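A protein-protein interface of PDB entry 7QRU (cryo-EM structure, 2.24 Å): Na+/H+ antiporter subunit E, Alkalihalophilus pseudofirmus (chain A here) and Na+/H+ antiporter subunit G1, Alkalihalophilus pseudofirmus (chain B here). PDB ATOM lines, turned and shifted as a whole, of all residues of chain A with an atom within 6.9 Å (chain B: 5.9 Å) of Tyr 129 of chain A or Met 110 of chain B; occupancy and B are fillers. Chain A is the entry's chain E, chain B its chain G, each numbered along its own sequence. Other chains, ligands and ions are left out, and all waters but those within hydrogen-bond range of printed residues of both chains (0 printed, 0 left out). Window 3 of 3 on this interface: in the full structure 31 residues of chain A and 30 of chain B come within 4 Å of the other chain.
O of Ile 90 of chain A lies within hydrogen-bond range of N of Asp 106 of chain B (2.9 Å). N of Ala 92 of chain A is in hydrogen-bond range of OD2 of Asp 106 of chain B (3.0 Å). The side-chain carboxylate of Asp 120 of chain A sits at hydrogen-bond distance from the side-chain hydroxyl of Tyr 111 of chain B, at 2.5 Å. The side-chain hydroxyl of Tyr 129 of chain A sits close to the side-chain sulfur of Met 110 of chain B (3.7 Å).
The backbone carbonyl oxygen (O) of Val 91 of chain A is in hydrogen-bond range of the backbone NH (N) of Ile 130 of chain A (2.8 Å). The backbone NH of Met 119 of chain A sits at hydrogen-bond distance from the backbone carbonyl oxygen of Tyr 129 of chain A (2.9 Å). The backbone carbonyl oxygen of Asp 120 of chain A sits at hydrogen-bond distance from the backbone NH of Tyr 129 of chain A (2.8 Å).
Among the printed residues, merely in contact across the chains: Ile 90 of chain A with Leu 107 of chain B (3.6 Å), Val 91 of chain A with Asp 106 of chain B (3.6 Å), Tyr 129 of chain A with Leu 107 of chain B (3.6 Å), Asp 120 of chain A with Met 110 of chain B (3.7 Å), Tyr 129 of chain A with Asp 106 of chain B (3.7 Å) and Asp 120 of chain A with Leu 107 of chain B (3.9 Å).
Of the 17 printed residues of chain A, 5 touch a printed residue of chain B. Printed residues of chain A that touch a printed residue of chain B: Ile 90, Val 91, Ala 92, Asp 120 and Tyr 129. Hydrophobic or aromatic side chains of chain A within 4 Å of the printed part of chain B: Ile 90 and Tyr 129. Among the printed residues, 10 pairs touch across the chains. Among the printed residues, no Asp or Glu carboxylate lies within 4 Å of a Lys or Arg side-chain nitrogen of the other chain.
Tyr 129 of chain A touches three residues of chain B. Of the printed residues of chain A, Tyr 111 of chain B touches Asp 120 (2.5 Å). Printed residues of chain B within 4 Å of Asp 120 of chain A: Leu 107 (3.9 Å), Met 110 (3.7 Å) and Tyr 111 (2.5 Å). Of the printed residues of chain B, Ala 92 of chain A touches Asp 106. Of the printed residues of chain B, Ile 90 of chain A touches Asp 106 (2.9 Å) and Leu 107 (3.6 Å). Of the printed residues of chain A, Leu 107 of chain B touches Ile 90 (3.6 Å), Asp 120 (3.9 Å) and Tyr 129 (3.6 Å). Lys 109 of chain B touches none of the printed residues of chain A. Ser 118 of chain A touches none of the printed residues of chain B. The nearest printed residue of chain B that does not touch Tyr 129 of chain A is Lys 108 of chain B (6.1 Å). The nearest printed residue of chain B that does not touch Ile 90 of chain A is Lys 108 of chain B (6.2 Å).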
ATOM      1  N   ILE A  90     -12.236 -23.882  21.684  1.00  0.00           N
ATOM      2  CA  ILE A  90     -10.965 -23.545  21.057  1.00  0.00           C
ATOM      3  C   ILE A  90     -10.860 -22.058  20.779  1.00  0.00           C
ATOM      4  O   ILE A  90     -11.677 -21.551  20.093  1.00  0.00           O
ATOM      5  CB  ILE A  90     -10.670 -24.357  19.794  1.00  0.00           C
ATOM      6  CG1 ILE A  90     -10.796 -25.844  20.094  1.00  0.00           C
ATOM      7  CG2 ILE A  90      -9.265 -24.019  19.251  1.00  0.00           C
ATOM      8  CD1 ILE A  90     -10.292 -26.809  19.134  1.00  0.00           C
ATOM      9  N   VAL A  91      -9.865 -21.373  21.377  1.00  0.00           N
ATOM     10  CA  VAL A  91      -9.691 -19.935  21.269  1.00  0.00           C
ATOM     11  C   VAL A  91      -8.456 -19.624  20.448  1.00  0.00           C
ATOM     12  O   VAL A  91      -7.396 -20.127  20.812  1.00  0.00           O
ATOM     13  CB  VAL A  91      -9.543 -19.329  22.675  1.00  0.00           C
ATOM     14  CG1 VAL A  91      -9.491 -17.853  22.654  1.00  0.00           C
ATOM     15  CG2 VAL A  91     -10.728 -19.722  23.468  1.00  0.00           C
ATOM     16  N   ALA A  92      -8.543 -18.726  19.447  1.00  0.00           N
ATOM     17  CA  ALA A  92      -7.318 -18.243  18.815  1.00  0.00           C
ATOM     18  C   ALA A  92      -6.694 -17.123  19.665  1.00  0.00           C
ATOM     19  O   ALA A  92      -7.386 -16.203  20.037  1.00  0.00           O
ATOM     20  CB  ALA A  92      -7.551 -17.818  17.420  1.00  0.00           C
ATOM     21  N   VAL A  93      -5.438 -17.261  20.057  1.00  0.00           N
ATOM     22  CA  VAL A  93      -4.761 -16.263  20.886  1.00  0.00           C
ATOM     23  C   VAL A  93      -3.584 -15.641  20.106  1.00  0.00           C
ATOM     24  O   VAL A  93      -2.645 -16.328  19.702  1.00  0.00           O
ATOM     25  CB  VAL A  93      -4.265 -16.880  22.194  1.00  0.00           C
ATOM     26  CG1 VAL A  93      -3.505 -15.886  22.999  1.00  0.00           C
ATOM     27  CG2 VAL A  93      -5.407 -17.470  22.974  1.00  0.00           C
ATOM     28  N   ILE A 110       1.866 -22.899  27.704  1.00  0.00           N
ATOM     29  CA  ILE A 110       0.419 -22.919  27.676  1.00  0.00           C
ATOM     30  C   ILE A 110      -0.134 -24.305  28.025  1.00  0.00           C
ATOM     31  O   ILE A 110      -1.138 -24.459  28.719  1.00  0.00           O
ATOM     32  CB  ILE A 110      -0.026 -22.382  26.304  1.00  0.00           C
ATOM     33  CG1 ILE A 110       0.182 -20.869  26.280  1.00  0.00           C
ATOM     34  CG2 ILE A 110      -1.479 -22.688  25.997  1.00  0.00           C
ATOM     35  CD1 ILE A 110       0.034 -20.263  24.946  1.00  0.00           C
ATOM     36  N   LEU A 117      -4.585 -25.990  26.659  1.00  0.00           N
ATOM     37  CA  LEU A 117      -3.764 -26.887  25.898  1.00  0.00           C
ATOM     38  C   LEU A 117      -3.568 -26.368  24.484  1.00  0.00           C
ATOM     39  O   LEU A 117      -4.555 -26.162  23.832  1.00  0.00           O
ATOM     40  CB  LEU A 117      -4.582 -28.148  25.872  1.00  0.00           C
ATOM     41  CG  LEU A 117      -3.831 -29.386  25.510  1.00  0.00           C
ATOM     42  CD1 LEU A 117      -3.169 -29.921  26.771  1.00  0.00           C
ATOM     43  CD2 LEU A 117      -4.827 -30.347  24.915  1.00  0.00           C
ATOM     44  N   SER A 118      -2.325 -26.244  24.034  1.00  0.00           N
ATOM     45  CA  SER A 118      -1.946 -25.783  22.710  1.00  0.00           C
ATOM     46  C   SER A 118      -2.363 -26.823  21.711  1.00  0.00           C
ATOM     47  O   SER A 118      -1.871 -27.969  21.783  1.00  0.00           O
ATOM     48  CB  SER A 118      -0.437 -25.495  22.578  1.00  0.00           C
ATOM     49  OG  SER A 118       0.028 -24.594  23.555  1.00  0.00           O
ATOM     50  N   MET A 119      -3.272 -26.449  20.801  1.00  0.00           N
ATOM     51  CA  MET A 119      -3.721 -27.333  19.718  1.00  0.00           C
ATOM     52  C   MET A 119      -2.861 -27.187  18.441  1.00  0.00           C
ATOM     53  O   MET A 119      -2.424 -28.137  17.853  1.00  0.00           O
ATOM     54  CB  MET A 119      -5.154 -26.974  19.338  1.00  0.00           C
ATOM     55  CG  MET A 119      -6.173 -27.236  20.400  1.00  0.00           C
ATOM     56  SD  MET A 119      -6.896 -28.832  20.114  1.00  0.00           S
ATOM     57  CE  MET A 119      -5.745 -29.809  21.085  1.00  0.00           C
ATOM     58  N   ASP A 120      -2.617 -25.977  17.994  1.00  0.00           N
ATOM     59  CA  ASP A 120      -2.233 -25.692  16.638  1.00  0.00           C
ATOM     60  C   ASP A 120      -1.707 -24.274  16.565  1.00  0.00           C
ATOM     61  O   ASP A 120      -1.943 -23.529  17.474  1.00  0.00           O
ATOM     62  CB  ASP A 120      -3.350 -25.769  15.592  1.00  0.00           C
ATOM     63  CG  ASP A 120      -2.927 -26.247  14.177  1.00  0.00           C
ATOM     64  OD1 ASP A 120      -1.668 -26.359  13.806  1.00  0.00           O
ATOM     65  OD2 ASP A 120      -3.801 -26.712  13.508  1.00  0.00           O
ATOM     66  N   PHE A 121      -1.002 -23.960  15.471  1.00  0.00           N
ATOM     67  CA  PHE A 121      -0.453 -22.635  15.211  1.00  0.00           C
ATOM     68  C   PHE A 121      -1.020 -22.199  13.895  1.00  0.00           C
ATOM     69  O   PHE A 121      -1.126 -23.066  13.039  1.00  0.00           O
ATOM     70  CB  PHE A 121       1.072 -22.675  15.100  1.00  0.00           C
ATOM     71  CG  PHE A 121       1.835 -22.586  16.400  1.00  0.00           C
ATOM     72  CD1 PHE A 121       1.876 -21.363  17.020  1.00  0.00           C
ATOM     73  CD2 PHE A 121       2.313 -23.710  17.087  1.00  0.00           C
ATOM     74  CE1 PHE A 121       2.584 -21.206  18.194  1.00  0.00           C
ATOM     75  CE2 PHE A 121       2.999 -23.549  18.285  1.00  0.00           C
ATOM     76  CZ  PHE A 121       3.197 -22.291  18.778  1.00  0.00           C
ATOM     77  N   SER A 122      -1.312 -20.906  13.707  1.00  0.00           N
ATOM     78  CA  SER A 122      -1.623 -20.454  12.338  1.00  0.00           C
ATOM     79  C   SER A 122      -0.422 -20.634  11.386  1.00  0.00           C
ATOM     80  O   SER A 122       0.740 -20.714  11.833  1.00  0.00           O
ATOM     81  CB  SER A 122      -2.119 -19.028  12.363  1.00  0.00           C
ATOM     82  OG  SER A 122      -1.214 -18.183  12.980  1.00  0.00           O
ATOM     83  N   ASP A 123      -0.668 -20.565  10.089  1.00  0.00           N
ATOM     84  CA  ASP A 123       0.406 -20.722   9.118  1.00  0.00           C
ATOM     85  C   ASP A 123       1.459 -19.620   9.286  1.00  0.00           C
ATOM     86  O   ASP A 123       2.659 -19.843   9.191  1.00  0.00           O
ATOM     87  CB  ASP A 123      -0.164 -20.801   7.701  1.00  0.00           C
ATOM     88  CG  ASP A 123      -0.774 -22.167   7.380  1.00  0.00           C
ATOM     89  OD1 ASP A 123      -1.824 -22.223   6.654  1.00  0.00           O
ATOM     90  OD2 ASP A 123      -0.196 -23.183   7.856  1.00  0.00           O
ATOM     91  N   TYR A 127      -1.019 -16.709  15.525  1.00  0.00           N
ATOM     92  CA  TYR A 127      -2.038 -17.187  16.457  1.00  0.00           C
ATOM     93  C   TYR A 127      -1.668 -18.560  16.986  1.00  0.00           C
ATOM     94  O   TYR A 127      -1.198 -19.399  16.191  1.00  0.00           O
ATOM     95  CB  TYR A 127      -3.411 -17.232  15.775  1.00  0.00           C
ATOM     96  CG  TYR A 127      -4.057 -15.884  15.585  1.00  0.00           C
ATOM     97  CD1 TYR A 127      -3.816 -15.138  14.452  1.00  0.00           C
ATOM     98  CD2 TYR A 127      -4.853 -15.325  16.539  1.00  0.00           C
ATOM     99  CE1 TYR A 127      -4.299 -13.859  14.286  1.00  0.00           C
ATOM    100  CE2 TYR A 127      -5.400 -14.076  16.357  1.00  0.00           C
ATOM    101  CZ  TYR A 127      -5.135 -13.338  15.231  1.00  0.00           C
ATOM    102  OH  TYR A 127      -5.668 -12.080  15.038  1.00  0.00           O
ATOM    103  N   ILE A 128      -1.965 -18.786  18.286  1.00  0.00           N
ATOM    104  CA  ILE A 128      -1.805 -20.119  18.857  1.00  0.00           C
ATOM    105  C   ILE A 128      -3.217 -20.543  19.203  1.00  0.00           C
ATOM    106  O   ILE A 128      -3.877 -19.918  19.976  1.00  0.00           O
ATOM    107  CB  ILE A 128      -0.765 -20.148  19.992  1.00  0.00           C
ATOM    108  CG1 ILE A 128      -0.812 -21.429  20.782  1.00  0.00           C
ATOM    109  CG2 ILE A 128      -1.060 -18.979  20.935  1.00  0.00           C
ATOM    110  CD1 ILE A 128      -0.271 -22.593  20.133  1.00  0.00           C
ATOM    111  N   TYR A 129      -3.684 -21.633  18.606  1.00  0.00           N
ATOM    112  CA  TYR A 129      -5.040 -22.174  18.907  1.00  0.00           C
ATOM    113  C   TYR A 129      -5.051 -22.929  20.233  1.00  0.00           C
ATOM    114  O   TYR A 129      -4.177 -23.749  20.431  1.00  0.00           O
ATOM    115  CB  TYR A 129      -5.603 -23.024  17.762  1.00  0.00           C
ATOM    116  CG  TYR A 129      -5.915 -22.145  16.574  1.00  0.00           C
ATOM    117  CD1 TYR A 129      -7.152 -21.553  16.387  1.00  0.00           C
ATOM    118  CD2 TYR A 129      -4.878 -21.752  15.742  1.00  0.00           C
ATOM    119  CE1 TYR A 129      -7.328 -20.675  15.339  1.00  0.00           C
ATOM    120  CE2 TYR A 129      -5.036 -20.846  14.728  1.00  0.00           C
ATOM    121  CZ  TYR A 129      -6.278 -20.337  14.496  1.00  0.00           C
ATOM    122  OH  TYR A 129      -6.402 -19.487  13.425  1.00  0.00           O
ATOM    123  N   ILE A 130      -5.882 -22.496  21.191  1.00  0.00           N
ATOM    124  CA  ILE A 130      -5.858 -23.086  22.519  1.00  0.00           C
ATOM    125  C   ILE A 130      -7.166 -23.778  22.939  1.00  0.00           C
ATOM    126  O   ILE A 130      -8.206 -23.158  22.948  1.00  0.00           O
ATOM    127  CB  ILE A 130      -5.409 -21.987  23.461  1.00  0.00           C
ATOM    128  CG1 ILE A 130      -4.001 -21.544  23.092  1.00  0.00           C
ATOM    129  CG2 ILE A 130      -5.467 -22.448  24.895  1.00  0.00           C
ATOM    130  CD1 ILE A 130      -3.626 -20.330  23.954  1.00  0.00           C
ATOM    131  N   HIS A 131      -7.075 -25.076  23.286  1.00  0.00           N
ATOM    132  CA  HIS A 131      -8.210 -25.762  23.828  1.00  0.00           C
ATOM    133  C   HIS A 131      -8.248 -25.378  25.294  1.00  0.00           C
ATOM    134  O   HIS A 131      -7.280 -25.641  25.971  1.00  0.00           O
ATOM    135  CB  HIS A 131      -8.173 -27.261  23.686  1.00  0.00           C
ATOM    136  CG  HIS A 131      -9.431 -27.894  24.150  1.00  0.00           C
ATOM    137  ND1 HIS A 131      -9.604 -28.437  25.420  1.00  0.00           N
ATOM    138  CD2 HIS A 131     -10.579 -28.075  23.482  1.00  0.00           C
ATOM    139  CE1 HIS A 131     -10.869 -28.792  25.558  1.00  0.00           C
ATOM    140  NE2 HIS A 131     -11.462 -28.652  24.366  1.00  0.00           N
ATOM    141  N   ASP B 106     -12.597 -21.707  17.347  1.00  0.00           N
ATOM    142  CA  ASP B 106     -11.902 -20.821  16.416  1.00  0.00           C
ATOM    143  C   ASP B 106     -11.112 -21.570  15.344  1.00  0.00           C
ATOM    144  O   ASP B 106     -10.855 -21.034  14.285  1.00  0.00           O
ATOM    145  CB  ASP B 106     -11.073 -19.800  17.163  1.00  0.00           C
ATOM    146  CG  ASP B 106     -11.934 -18.797  17.943  1.00  0.00           C
ATOM    147  OD1 ASP B 106     -13.209 -18.795  17.747  1.00  0.00           O
ATOM    148  OD2 ASP B 106     -11.349 -17.982  18.752  1.00  0.00           O
ATOM    149  N   LEU B 107     -10.721 -22.787  15.655  1.00  0.00           N
ATOM    150  CA  LEU B 107      -9.904 -23.638  14.833  1.00  0.00           C
ATOM    151  C   LEU B 107     -10.701 -24.184  13.643  1.00  0.00           C
ATOM    152  O   LEU B 107     -10.147 -24.533  12.634  1.00  0.00           O
ATOM    153  CB  LEU B 107      -9.390 -24.760  15.754  1.00  0.00           C
ATOM    154  CG  LEU B 107      -8.379 -25.696  15.089  1.00  0.00           C
ATOM    155  CD1 LEU B 107      -7.105 -24.944  14.639  1.00  0.00           C
ATOM    156  CD2 LEU B 107      -7.975 -26.734  16.032  1.00  0.00           C
ATOM    157  N   LYS B 108     -12.003 -24.271  13.742  1.00  0.00           N
ATOM    158  CA  LYS B 108     -12.847 -24.762  12.672  1.00  0.00           C
ATOM    159  C   LYS B 108     -12.707 -23.852  11.467  1.00  0.00           C
ATOM    160  O   LYS B 108     -12.637 -24.321  10.336  1.00  0.00           O
ATOM    161  CB  LYS B 108     -14.316 -24.751  13.112  1.00  0.00           C
ATOM    162  CG  LYS B 108     -15.293 -25.408  12.164  1.00  0.00           C
ATOM    163  CD  LYS B 108     -16.704 -25.577  12.708  1.00  0.00           C
ATOM    164  CE  LYS B 108     -17.362 -24.243  13.023  1.00  0.00           C
ATOM    165  NZ  LYS B 108     -17.097 -23.738  14.403  1.00  0.00           N
ATOM    166  N   LYS B 109     -12.735 -22.542  11.739  1.00  0.00           N
ATOM    167  CA  LYS B 109     -12.582 -21.545  10.675  1.00  0.00           C
ATOM    168  C   LYS B 109     -11.289 -21.827   9.914  1.00  0.00           C
ATOM    169  O   LYS B 109     -11.315 -22.170   8.724  1.00  0.00           O
ATOM    170  CB  LYS B 109     -12.578 -20.111  11.210  1.00  0.00           C
ATOM    171  CG  LYS B 109     -13.595 -19.846  12.306  1.00  0.00           C
ATOM    172  CD  LYS B 109     -14.994 -20.156  11.837  1.00  0.00           C
ATOM    173  CE  LYS B 109     -16.067 -19.677  12.792  1.00  0.00           C
ATOM    174  NZ  LYS B 109     -16.388 -20.689  13.827  1.00  0.00           N
ATOM    175  N   MET B 110     -10.170 -21.702  10.625  1.00  0.00           N
ATOM    176  CA  MET B 110      -8.861 -21.951  10.046  1.00  0.00           C
ATOM    177  C   MET B 110      -8.898 -23.206   9.173  1.00  0.00           C
ATOM    178  O   MET B 110      -8.515 -23.132   8.004  1.00  0.00           O
ATOM    179  CB  MET B 110      -7.783 -22.100  11.128  1.00  0.00           C
ATOM    180  CG  MET B 110      -6.386 -21.904  10.602  1.00  0.00           C
ATOM    181  SD  MET B 110      -5.060 -22.478  11.635  1.00  0.00           S
ATOM    182  CE  MET B 110      -4.994 -24.185  11.139  1.00  0.00           C
ATOM    183  N   TYR B 111      -9.387 -24.348   9.685  1.00  0.00           N
ATOM    184  CA  TYR B 111      -9.414 -25.566   8.860  1.00  0.00           C
ATOM    185  C   TYR B 111     -10.484 -25.518   7.759  1.00  0.00           C
ATOM    186  O   TYR B 111     -10.629 -26.495   7.022  1.00  0.00           O
ATOM    187  CB  TYR B 111      -9.643 -26.857   9.668  1.00  0.00           C
ATOM    188  CG  TYR B 111      -8.355 -27.323  10.263  1.00  0.00           C
ATOM    189  CD1 TYR B 111      -7.415 -27.927   9.459  1.00  0.00           C
ATOM    190  CD2 TYR B 111      -8.000 -26.950  11.536  1.00  0.00           C
ATOM    191  CE1 TYR B 111      -6.160 -28.213   9.938  1.00  0.00           C
ATOM    192  CE2 TYR B 111      -6.756 -27.246  12.037  1.00  0.00           C
ATOM    193  CZ  TYR B 111      -5.833 -27.872  11.238  1.00  0.00           C
ATOM    194  OH  TYR B 111      -4.611 -28.226  11.753  1.00  0.00           O
ATOM    195  N   GLU B 112     -11.258 -24.412   7.654  1.00  0.00           N
ATOM    196  CA  GLU B 112     -12.169 -24.182   6.527  1.00  0.00           C
ATOM    197  C   GLU B 112     -11.381 -23.783   5.261  1.00  0.00           C
ATOM    198  O   GLU B 112     -11.777 -24.135   4.137  1.00  0.00           O
ATOM    199  CB  GLU B 112     -13.284 -23.200   6.928  1.00  0.00           C
ATOM    200  CG  GLU B 112     -14.507 -23.984   7.471  1.00  0.00           C
ATOM    201  CD  GLU B 112     -15.510 -23.300   8.398  1.00  0.00           C
ATOM    202  OE1 GLU B 112     -15.493 -22.042   8.463  1.00  0.00           O
ATOM    203  OE2 GLU B 112     -16.299 -24.032   9.089  1.00  0.00           O
ATOM    204  N   LYS B 113     -10.233 -23.093   5.448  1.00  0.00           N
ATOM    205  CA  LYS B 113      -9.345 -22.635   4.375  1.00  0.00           C
ATOM    206  C   LYS B 113      -8.262 -23.696   4.074  1.00  0.00           C
ATOM    207  O   LYS B 113      -8.612 -24.805   3.551  1.00  0.00           O
ATOM    208  CB  LYS B 113      -8.684 -21.303   4.767  1.00  0.00           C
ATOM    209  CG  LYS B 113      -9.515 -20.351   5.625  1.00  0.00           C
ATOM    210  CD  LYS B 113     -10.846 -19.957   5.025  1.00  0.00           C
ATOM    211  CE  LYS B 113     -11.705 -19.115   5.949  1.00  0.00           C
ATOM    212  NZ  LYS B 113     -12.594 -19.938   6.806  1.00  0.00           N
